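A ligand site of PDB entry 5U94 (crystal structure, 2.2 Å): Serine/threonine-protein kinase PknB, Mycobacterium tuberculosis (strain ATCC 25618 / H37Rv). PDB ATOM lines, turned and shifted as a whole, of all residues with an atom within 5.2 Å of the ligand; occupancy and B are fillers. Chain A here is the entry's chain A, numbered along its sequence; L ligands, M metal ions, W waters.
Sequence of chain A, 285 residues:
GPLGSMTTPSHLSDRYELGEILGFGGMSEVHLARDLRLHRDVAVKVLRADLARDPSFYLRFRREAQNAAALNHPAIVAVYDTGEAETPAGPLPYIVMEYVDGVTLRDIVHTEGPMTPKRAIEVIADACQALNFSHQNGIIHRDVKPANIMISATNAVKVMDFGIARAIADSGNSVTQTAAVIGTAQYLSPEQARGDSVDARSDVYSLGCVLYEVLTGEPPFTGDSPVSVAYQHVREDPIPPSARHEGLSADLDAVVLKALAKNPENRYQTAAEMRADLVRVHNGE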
ATOM      1  N   LEU A  22      -2.069 -23.645  -4.604  1.00  0.00           N
ATOM      2  CA  LEU A  22      -0.616 -23.695  -4.688  1.00  0.00           C
ATOM      3  C   LEU A  22       0.033 -22.323  -4.767  1.00  0.00           C
ATOM      4  O   LEU A  22       1.153 -22.147  -4.284  1.00  0.00           O
ATOM      5  CB  LEU A  22      -0.185 -24.515  -5.925  1.00  0.00           C
ATOM      6  CG  LEU A  22      -0.646 -25.965  -5.970  1.00  0.00           C
ATOM      7  CD1 LEU A  22      -0.246 -26.609  -7.299  1.00  0.00           C
ATOM      8  CD2 LEU A  22      -0.072 -26.760  -4.804  1.00  0.00           C
ATOM      9  N   GLY A  23      -0.649 -21.348  -5.351  1.00  0.00           N
ATOM     10  CA  GLY A  23      -0.122 -19.993  -5.459  1.00  0.00           C
ATOM     11  C   GLY A  23      -1.156 -19.098  -6.089  1.00  0.00           C
ATOM     12  O   GLY A  23      -2.160 -19.566  -6.644  1.00  0.00           O
ATOM     13  N   PHE A  24      -0.911 -17.800  -5.986  1.00  0.00           N
ATOM     14  CA  PHE A  24      -1.826 -16.827  -6.570  1.00  0.00           C
ATOM     15  C   PHE A  24      -1.084 -15.518  -6.836  1.00  0.00           C
ATOM     16  O   PHE A  24      -0.089 -15.219  -6.178  1.00  0.00           O
ATOM     17  CB  PHE A  24      -3.035 -16.577  -5.667  1.00  0.00           C
ATOM     18  CG  PHE A  24      -2.696 -15.937  -4.352  1.00  0.00           C
ATOM     19  CD1 PHE A  24      -2.758 -14.562  -4.193  1.00  0.00           C
ATOM     20  CD2 PHE A  24      -2.338 -16.714  -3.267  1.00  0.00           C
ATOM     21  CE1 PHE A  24      -2.450 -13.974  -2.991  1.00  0.00           C
ATOM     22  CE2 PHE A  24      -2.021 -16.125  -2.051  1.00  0.00           C
ATOM     23  CZ  PHE A  24      -2.083 -14.753  -1.906  1.00  0.00           C
ATOM     24  N   GLY A  25      -1.585 -14.779  -7.809  1.00  0.00           N
ATOM     25  CA  GLY A  25      -1.072 -13.458  -8.113  1.00  0.00           C
ATOM     26  C   GLY A  25      -2.182 -12.412  -8.104  1.00  0.00           C
ATOM     27  O   GLY A  25      -3.154 -12.562  -7.364  1.00  0.00           O
ATOM     28  N   VAL A  30      -3.621 -20.624  -8.814  1.00  0.00           N
ATOM     29  CA  VAL A  30      -3.264 -21.961  -9.280  1.00  0.00           C
ATOM     30  C   VAL A  30      -3.614 -22.950  -8.177  1.00  0.00           C
ATOM     31  O   VAL A  30      -3.088 -22.860  -7.063  1.00  0.00           O
ATOM     32  CB  VAL A  30      -1.771 -22.061  -9.649  1.00  0.00           C
ATOM     33  CG1 VAL A  30      -1.408 -23.477 -10.071  1.00  0.00           C
ATOM     34  CG2 VAL A  30      -1.452 -21.087 -10.778  1.00  0.00           C
ATOM     35  N   ALA A  43      -2.442 -29.387 -12.163  1.00  0.00           N
ATOM     36  CA  ALA A  43      -2.544 -28.024 -11.665  1.00  0.00           C
ATOM     37  C   ALA A  43      -3.455 -27.235 -12.582  1.00  0.00           C
ATOM     38  O   ALA A  43      -3.423 -27.421 -13.812  1.00  0.00           O
ATOM     39  CB  ALA A  43      -1.162 -27.355 -11.576  1.00  0.00           C
ATOM     40  N   LYS A  45      -4.716 -23.335 -13.493  1.00  0.00           N
ATOM     41  CA  LYS A  45      -4.572 -21.892 -13.391  1.00  0.00           C
ATOM     42  C   LYS A  45      -5.908 -21.246 -13.761  1.00  0.00           C
ATOM     43  O   LYS A  45      -6.438 -21.497 -14.852  1.00  0.00           O
ATOM     44  CB  LYS A  45      -3.459 -21.376 -14.311  1.00  0.00           C
ATOM     45  CG  LYS A  45      -2.999 -19.969 -13.992  1.00  0.00           C
ATOM     46  CD  LYS A  45      -1.788 -19.588 -14.818  1.00  0.00           C
ATOM     47  CE  LYS A  45      -1.113 -18.361 -14.272  1.00  0.00           C
ATOM     48  NZ  LYS A  45       0.078 -17.963 -15.066  1.00  0.00           N
ATOM     49  N   GLU A  64      -1.831 -16.815 -23.139  1.00  0.00           N
ATOM     50  CA  GLU A  64      -0.912 -17.584 -22.306  1.00  0.00           C
ATOM     51  C   GLU A  64      -1.085 -19.084 -22.549  1.00  0.00           C
ATOM     52  O   GLU A  64      -0.106 -19.820 -22.720  1.00  0.00           O
ATOM     53  CB  GLU A  64      -1.130 -17.253 -20.834  1.00  0.00           C
ATOM     54  CG  GLU A  64      -0.346 -18.138 -19.868  1.00  0.00           C
ATOM     55  CD  GLU A  64      -0.578 -17.764 -18.405  1.00  0.00           C
ATOM     56  OE1 GLU A  64      -1.339 -16.804 -18.146  1.00  0.00           O
ATOM     57  OE2 GLU A  64      -0.002 -18.438 -17.535  1.00  0.00           O
ATOM     58  N   ALA A  68       1.966 -21.381 -24.216  1.00  0.00           N
ATOM     59  CA  ALA A  68       2.507 -22.489 -23.438  1.00  0.00           C
ATOM     60  C   ALA A  68       2.240 -23.823 -24.118  1.00  0.00           C
ATOM     61  O   ALA A  68       3.108 -24.709 -24.128  1.00  0.00           O
ATOM     62  CB  ALA A  68       1.925 -22.480 -22.032  1.00  0.00           C
ATOM     63  N   VAL A  77       6.693 -26.507 -18.171  1.00  0.00           N
ATOM     64  CA  VAL A  77       5.423 -27.025 -17.702  1.00  0.00           C
ATOM     65  C   VAL A  77       4.500 -27.229 -18.894  1.00  0.00           C
ATOM     66  O   VAL A  77       4.327 -26.330 -19.722  1.00  0.00           O
ATOM     67  CB  VAL A  77       4.817 -26.082 -16.652  1.00  0.00           C
ATOM     68  CG1 VAL A  77       3.434 -26.545 -16.211  1.00  0.00           C
ATOM     69  CG2 VAL A  77       5.736 -25.968 -15.437  1.00  0.00           C
ATOM     70  N   VAL A  79       0.943 -27.882 -20.907  1.00  0.00           N
ATOM     71  CA  VAL A  79      -0.479 -27.556 -20.874  1.00  0.00           C
ATOM     72  C   VAL A  79      -1.249 -28.742 -21.431  1.00  0.00           C
ATOM     73  O   VAL A  79      -0.936 -29.255 -22.513  1.00  0.00           O
ATOM     74  CB  VAL A  79      -0.775 -26.286 -21.675  1.00  0.00           C
ATOM     75  CG1 VAL A  79      -2.282 -26.033 -21.753  1.00  0.00           C
ATOM     76  CG2 VAL A  79      -0.078 -25.093 -21.064  1.00  0.00           C
ATOM     77  N   ILE A  95      -6.857 -22.949 -17.098  1.00  0.00           N
ATOM     78  CA  ILE A  95      -5.858 -23.699 -17.849  1.00  0.00           C
ATOM     79  C   ILE A  95      -5.454 -24.899 -17.008  1.00  0.00           C
ATOM     80  O   ILE A  95      -5.065 -24.758 -15.842  1.00  0.00           O
ATOM     81  CB  ILE A  95      -4.619 -22.839 -18.174  1.00  0.00           C
ATOM     82  CG1 ILE A  95      -5.021 -21.625 -19.017  1.00  0.00           C
ATOM     83  CG2 ILE A  95      -3.559 -23.657 -18.889  1.00  0.00           C
ATOM     84  CD1 ILE A  95      -3.928 -20.577 -19.152  1.00  0.00           C
ATOM     85  N   MET A  97      -2.814 -27.981 -16.503  1.00  0.00           N
ATOM     86  CA  MET A  97      -1.416 -28.169 -16.837  1.00  0.00           C
ATOM     87  C   MET A  97      -0.784 -29.244 -15.962  1.00  0.00           C
ATOM     88  O   MET A  97      -1.404 -29.756 -15.014  1.00  0.00           O
ATOM     89  CB  MET A  97      -0.636 -26.857 -16.692  1.00  0.00           C
ATOM     90  CG  MET A  97      -0.638 -26.300 -15.277  1.00  0.00           C
ATOM     91  SD  MET A  97      -0.247 -24.549 -15.233  1.00  0.00           S
ATOM     92  CE  MET A  97      -0.574 -24.172 -13.514  1.00  0.00           C
ATOM     93  N   GLU A  98       0.453 -29.570 -16.303  1.00  0.00           N
ATOM     94  CA  GLU A  98       1.250 -30.522 -15.540  1.00  0.00           C
ATOM     95  C   GLU A  98       1.438 -30.040 -14.098  1.00  0.00           C
ATOM     96  O   GLU A  98       1.729 -28.863 -13.864  1.00  0.00           O
ATOM     97  CB  GLU A  98       2.597 -30.711 -16.234  1.00  0.00           C
ATOM     98  CG  GLU A  98       3.708 -31.332 -15.394  1.00  0.00           C
ATOM     99  CD  GLU A  98       5.048 -31.293 -16.117  1.00  0.00           C
ATOM    100  OE1 GLU A  98       5.176 -30.539 -17.096  1.00  0.00           O
ATOM    101  OE2 GLU A  98       5.976 -32.013 -15.688  1.00  0.00           O
ATOM    102  N   TYR A  99       1.259 -30.951 -13.149  1.00  0.00           N
ATOM    103  CA  TYR A  99       1.521 -30.683 -11.745  1.00  0.00           C
ATOM    104  C   TYR A  99       2.980 -30.973 -11.431  1.00  0.00           C
ATOM    105  O   TYR A  99       3.453 -32.098 -11.638  1.00  0.00           O
ATOM    106  CB  TYR A  99       0.599 -31.508 -10.848  1.00  0.00           C
ATOM    107  CG  TYR A  99       0.959 -31.453  -9.379  1.00  0.00           C
ATOM    108  CD1 TYR A  99       1.100 -32.626  -8.645  1.00  0.00           C
ATOM    109  CD2 TYR A  99       1.152 -30.237  -8.730  1.00  0.00           C
ATOM    110  CE1 TYR A  99       1.435 -32.582  -7.297  1.00  0.00           C
ATOM    111  CE2 TYR A  99       1.487 -30.194  -7.382  1.00  0.00           C
ATOM    112  CZ  TYR A  99       1.629 -31.372  -6.676  1.00  0.00           C
ATOM    113  OH  TYR A  99       1.954 -31.337  -5.348  1.00  0.00           O
ATOM    114  N   VAL A 100       3.688 -29.970 -10.935  1.00  0.00           N
ATOM    115  CA  VAL A 100       5.069 -30.107 -10.480  1.00  0.00           C
ATOM    116  C   VAL A 100       5.031 -30.063  -8.956  1.00  0.00           C
ATOM    117  O   VAL A 100       4.695 -29.034  -8.367  1.00  0.00           O
ATOM    118  CB  VAL A 100       5.973 -28.994 -11.049  1.00  0.00           C
ATOM    119  CG1 VAL A 100       7.414 -29.214 -10.605  1.00  0.00           C
ATOM    120  CG2 VAL A 100       5.880 -28.959 -12.563  1.00  0.00           C
ATOM    121  N   LYS A 145      12.499 -15.298 -13.804  1.00  0.00           N
ATOM    122  CA  LYS A 145      12.845 -14.878 -12.455  1.00  0.00           C
ATOM    123  C   LYS A 145      12.808 -16.102 -11.550  1.00  0.00           C
ATOM    124  O   LYS A 145      12.241 -17.131 -11.922  1.00  0.00           O
ATOM    125  CB  LYS A 145      11.896 -13.785 -11.939  1.00  0.00           C
ATOM    126  CG  LYS A 145      10.431 -14.201 -11.905  1.00  0.00           C
ATOM    127  CD  LYS A 145       9.560 -13.055 -11.390  1.00  0.00           C
ATOM    128  CE  LYS A 145       8.103 -13.470 -11.305  1.00  0.00           C
ATOM    129  NZ  LYS A 145       7.227 -12.365 -10.818  1.00  0.00           N
ATOM    130  N   ALA A 147      11.032 -17.006  -9.153  1.00  0.00           N
ATOM    131  CA  ALA A 147       9.717 -17.534  -8.820  1.00  0.00           C
ATOM    132  C   ALA A 147       9.077 -18.308  -9.954  1.00  0.00           C
ATOM    133  O   ALA A 147       8.086 -19.019  -9.721  1.00  0.00           O
ATOM    134  CB  ALA A 147       8.789 -16.396  -8.391  1.00  0.00           C
ATOM    135  N   ASN A 148       9.612 -18.216 -11.164  1.00  0.00           N
ATOM    136  CA  ASN A 148       9.047 -18.895 -12.321  1.00  0.00           C
ATOM    137  C   ASN A 148       9.841 -20.130 -12.750  1.00  0.00           C
ATOM    138  O   ASN A 148       9.512 -20.726 -13.778  1.00  0.00           O
ATOM    139  CB  ASN A 148       8.945 -17.918 -13.500  1.00  0.00           C
ATOM    140  CG  ASN A 148       7.896 -16.857 -13.276  1.00  0.00           C
ATOM    141  OD1 ASN A 148       7.050 -16.993 -12.398  1.00  0.00           O
ATOM    142  ND2 ASN A 148       7.935 -15.806 -14.090  1.00  0.00           N
ATOM    143  N   MET A 150      10.950 -23.876 -11.282  1.00  0.00           N
ATOM    144  CA  MET A 150      10.675 -24.850 -10.230  1.00  0.00           C
ATOM    145  C   MET A 150      11.651 -26.018 -10.306  1.00  0.00           C
ATOM    146  O   MET A 150      12.236 -26.303 -11.351  1.00  0.00           O
ATOM    147  CB  MET A 150       9.242 -25.390 -10.337  1.00  0.00           C
ATOM    148  CG  MET A 150       8.172 -24.365 -10.007  1.00  0.00           C
ATOM    149  SD  MET A 150       6.546 -25.134  -9.775  1.00  0.00           S
ATOM    150  CE  MET A 150       6.804 -26.018  -8.242  1.00  0.00           C
ATOM    151  N   MET A 160       7.925 -22.028 -15.914  1.00  0.00           N
ATOM    152  CA  MET A 160       6.478 -21.883 -15.898  1.00  0.00           C
ATOM    153  C   MET A 160       6.114 -20.403 -16.042  1.00  0.00           C
ATOM    154  O   MET A 160       6.983 -19.547 -16.255  1.00  0.00           O
ATOM    155  CB  MET A 160       5.900 -22.469 -14.604  1.00  0.00           C
ATOM    156  CG  MET A 160       6.248 -21.650 -13.372  1.00  0.00           C
ATOM    157  SD  MET A 160       5.814 -22.489 -11.839  1.00  0.00           S
ATOM    158  CE  MET A 160       6.256 -21.225 -10.644  1.00  0.00           C
ATOM    159  N   ASP A 161       4.822 -20.116 -15.918  1.00  0.00           N
ATOM    160  CA  ASP A 161       4.265 -18.770 -15.999  1.00  0.00           C
ATOM    161  C   ASP A 161       4.690 -18.042 -17.281  1.00  0.00           C
ATOM    162  O   ASP A 161       5.530 -17.142 -17.237  1.00  0.00           O
ATOM    163  CB  ASP A 161       4.656 -17.936 -14.776  1.00  0.00           C
ATOM    164  CG  ASP A 161       3.712 -16.775 -14.554  1.00  0.00           C
ATOM    165  OD1 ASP A 161       2.915 -16.475 -15.468  1.00  0.00           O
ATOM    166  OD2 ASP A 161       3.756 -16.160 -13.458  1.00  0.00           O
ATOM    167  N   PHE A 162       4.084 -18.420 -18.409  1.00  0.00           N
ATOM    168  CA  PHE A 162       4.224 -17.688 -19.657  1.00  0.00           C
ATOM    169  C   PHE A 162       3.329 -16.460 -19.784  1.00  0.00           C
ATOM    170  O   PHE A 162       3.173 -15.911 -20.885  1.00  0.00           O
ATOM    171  CB  PHE A 162       4.136 -18.654 -20.839  1.00  0.00           C
ATOM    172  CG  PHE A 162       5.363 -19.507 -21.017  1.00  0.00           C
ATOM    173  CD1 PHE A 162       5.659 -20.511 -20.108  1.00  0.00           C
ATOM    174  CD2 PHE A 162       6.208 -19.312 -22.086  1.00  0.00           C
ATOM    175  CE1 PHE A 162       6.782 -21.293 -20.252  1.00  0.00           C
ATOM    176  CE2 PHE A 162       7.341 -20.098 -22.244  1.00  0.00           C
ATOM    177  CZ  PHE A 162       7.628 -21.092 -21.330  1.00  0.00           C
ATOM    178  N   GLY A 163       2.743 -16.011 -18.677  1.00  0.00           N
ATOM    179  CA  GLY A 163       1.630 -15.068 -18.677  1.00  0.00           C
ATOM    180  C   GLY A 163       1.860 -13.805 -19.490  1.00  0.00           C
ATOM    181  O   GLY A 163       0.889 -13.169 -19.897  1.00  0.00           O
HETATM  182  C1  LIG L   1       1.795 -21.284 -15.106  1.00  0.00           C
HETATM  183  N1  LIG L   1       2.589 -22.410 -10.561  1.00  0.00           N
HETATM  184  N2  LIG L   1       2.278 -23.246 -12.494  1.00  0.00           N
HETATM  185  C2  LIG L   1       2.063 -20.885 -13.662  1.00  0.00           C
HETATM  186  O1  LIG L   1       2.694 -19.494  -9.743  1.00  0.00           O
HETATM  187  N3  LIG L   1       2.087 -19.578 -13.402  1.00  0.00           N
HETATM  188  C3  LIG L   1       2.238 -21.765 -12.650  1.00  0.00           C
HETATM  189  N4  LIG L   1       2.197 -26.220 -12.969  1.00  0.00           N
HETATM  190  C4  LIG L   1       2.435 -26.184 -11.544  1.00  0.00           C
HETATM  191  N5  LIG L   1       2.561 -27.170 -10.795  1.00  0.00           N
HETATM  192  O2  LIG L   1       2.785 -26.701  -9.479  1.00  0.00           O
HETATM  193  N6  LIG L   1       2.790 -25.293  -9.519  1.00  0.00           N
HETATM  194  C5  LIG L   1       2.591 -24.941 -10.699  1.00  0.00           C
HETATM  195  C6  LIG L   1       2.504 -23.514 -11.228  1.00  0.00           C
HETATM  196  C7  LIG L   1       2.839 -22.294  -9.129  1.00  0.00           C
HETATM  197  C8  LIG L   1       1.588 -21.828  -8.390  1.00  0.00           C
HETATM  198  C9  LIG L   1       1.646 -21.508 -16.256  1.00  0.00           C
HETATM  199  C10 LIG L   1       1.549 -21.789 -17.754  1.00  0.00           C
HETATM  200  C11 LIG L   1       2.634 -22.793 -18.117  1.00  0.00           C
HETATM  201  C12 LIG L   1       0.170 -22.332 -18.111  1.00  0.00           C
HETATM  202  O3  LIG L   1       1.773 -20.597 -18.445  1.00  0.00           O
HETATM  203  C13 LIG L   1       2.460 -21.306 -11.304  1.00  0.00           C
HETATM  204  C14 LIG L   1       2.481 -19.955 -11.052  1.00  0.00           C
HETATM  205  C15 LIG L   1       2.278 -19.089 -12.163  1.00  0.00           C
HETATM  206  C16 LIG L   1       2.740 -18.102  -9.484  1.00  0.00           C
HETATM  207  C17 LIG L   1       3.939 -17.776  -8.595  1.00  0.00           C
HETATM  208  C18 LIG L   1       3.511 -17.949  -7.143  1.00  0.00           C
HETATM  209  N7  LIG L   1       2.999 -16.690  -6.631  1.00  0.00           N
HETATM  210  C19 LIG L   1       4.097 -15.763  -6.433  1.00  0.00           C
HETATM  211  C20 LIG L   1       4.895 -15.549  -7.716  1.00  0.00           C
HETATM  212  C21 LIG L   1       4.338 -16.330  -8.904  1.00  0.00           C
HETATM  213 MG    MG M   1       4.827 -15.936 -11.439  1.00  0.00          MG
HETATM  214  O   HOH W   1       1.731 -17.410  -4.167  1.00  0.00           O
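N6 of the ligand sits close to SD of Met 150 (3.8 Å). The side-chain sulfur of Met 160 lies close to a nitrogen (N1) of the ligand (3.5 Å). Leu 22 touches the ligand. Gly 23 touches the ligand. Val 30 touches the ligand. CB of Ala 43 touches C4 of the ligand (3.8 Å). Ala 68 touches the ligand (CB to C11, 3.99 Å). Val 77 touches the ligand (CG1 to N4, 3.5 Å). Tyr 99 touches the ligand (CA to N5, 3.8 Å). Asp 161 touches the ligand (CB to N3, 3.3 Å). 17 residues have an atom within 4 Å of the ligand: Leu 22, Gly 23, Phe 24, Val 30, Ala 43, Lys 45, Glu 64, Ala 68, Val 77, Met 97, Glu 98, Tyr 99, Val 100, Met 150, Met 160, Asp 161 and Phe 162. Along chain A the residues within 4 Å of the ligand span positions 22 to 162.
A nitrogen (N4) of the ligand is in hydrogen-bond range of the backbone carbonyl oxygen (O) of Glu 98, at 2.8 Å. The side-chain carboxylate (OE2) of Glu 64 lies within hydrogen-bond range of an oxygen (O3) of the ligand, 2.9 Å away. N5 of the ligand sits at hydrogen-bond distance from N of Val 100, 3.0 Å away. NZ of Lys 45 is in hydrogen-bond range of N3 of the ligand, 3.1 Å away. The side-chain sulfur (SD) of Met 97 lies close to a nitrogen (N4) of the ligand. N of Phe 162 lies within hydrogen-bond range of O3 of the ligand (3.2 Å). N7 of the ligand lies within hydrogen-bond range of O of Phe 24, 3.5 Å away.
The side-chain carboxylate (OE2) of Glu 64 lies within salt-bridge range of the side-chain amino group (NZ) of Lys 45 (2.5 Å). NZ of Lys 45 lies within salt-bridge range of OD1 of Asp 161. N of Ile 95 lies within hydrogen-bond range of O of Lys 45, at 2.7 Å. O of Ala 43 lies within hydrogen-bond range of N of Met 97. N of Gly 163 sits close to OD1 of Asp 161, 3.2 Å away. N of Met 160 is in hydrogen-bond range of O of Asn 148 (3.0 Å). O of Val 30 sits at hydrogen-bond distance from N of Leu 22 (2.8 Å). O of Gly 23 lies within hydrogen-bond range of N of Val 30.
Water W1 lies within hydrogen-bond range of a nitrogen (N7) of the ligand (2.9 Å) and the backbone NH of Phe 24 (3.2 Å).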
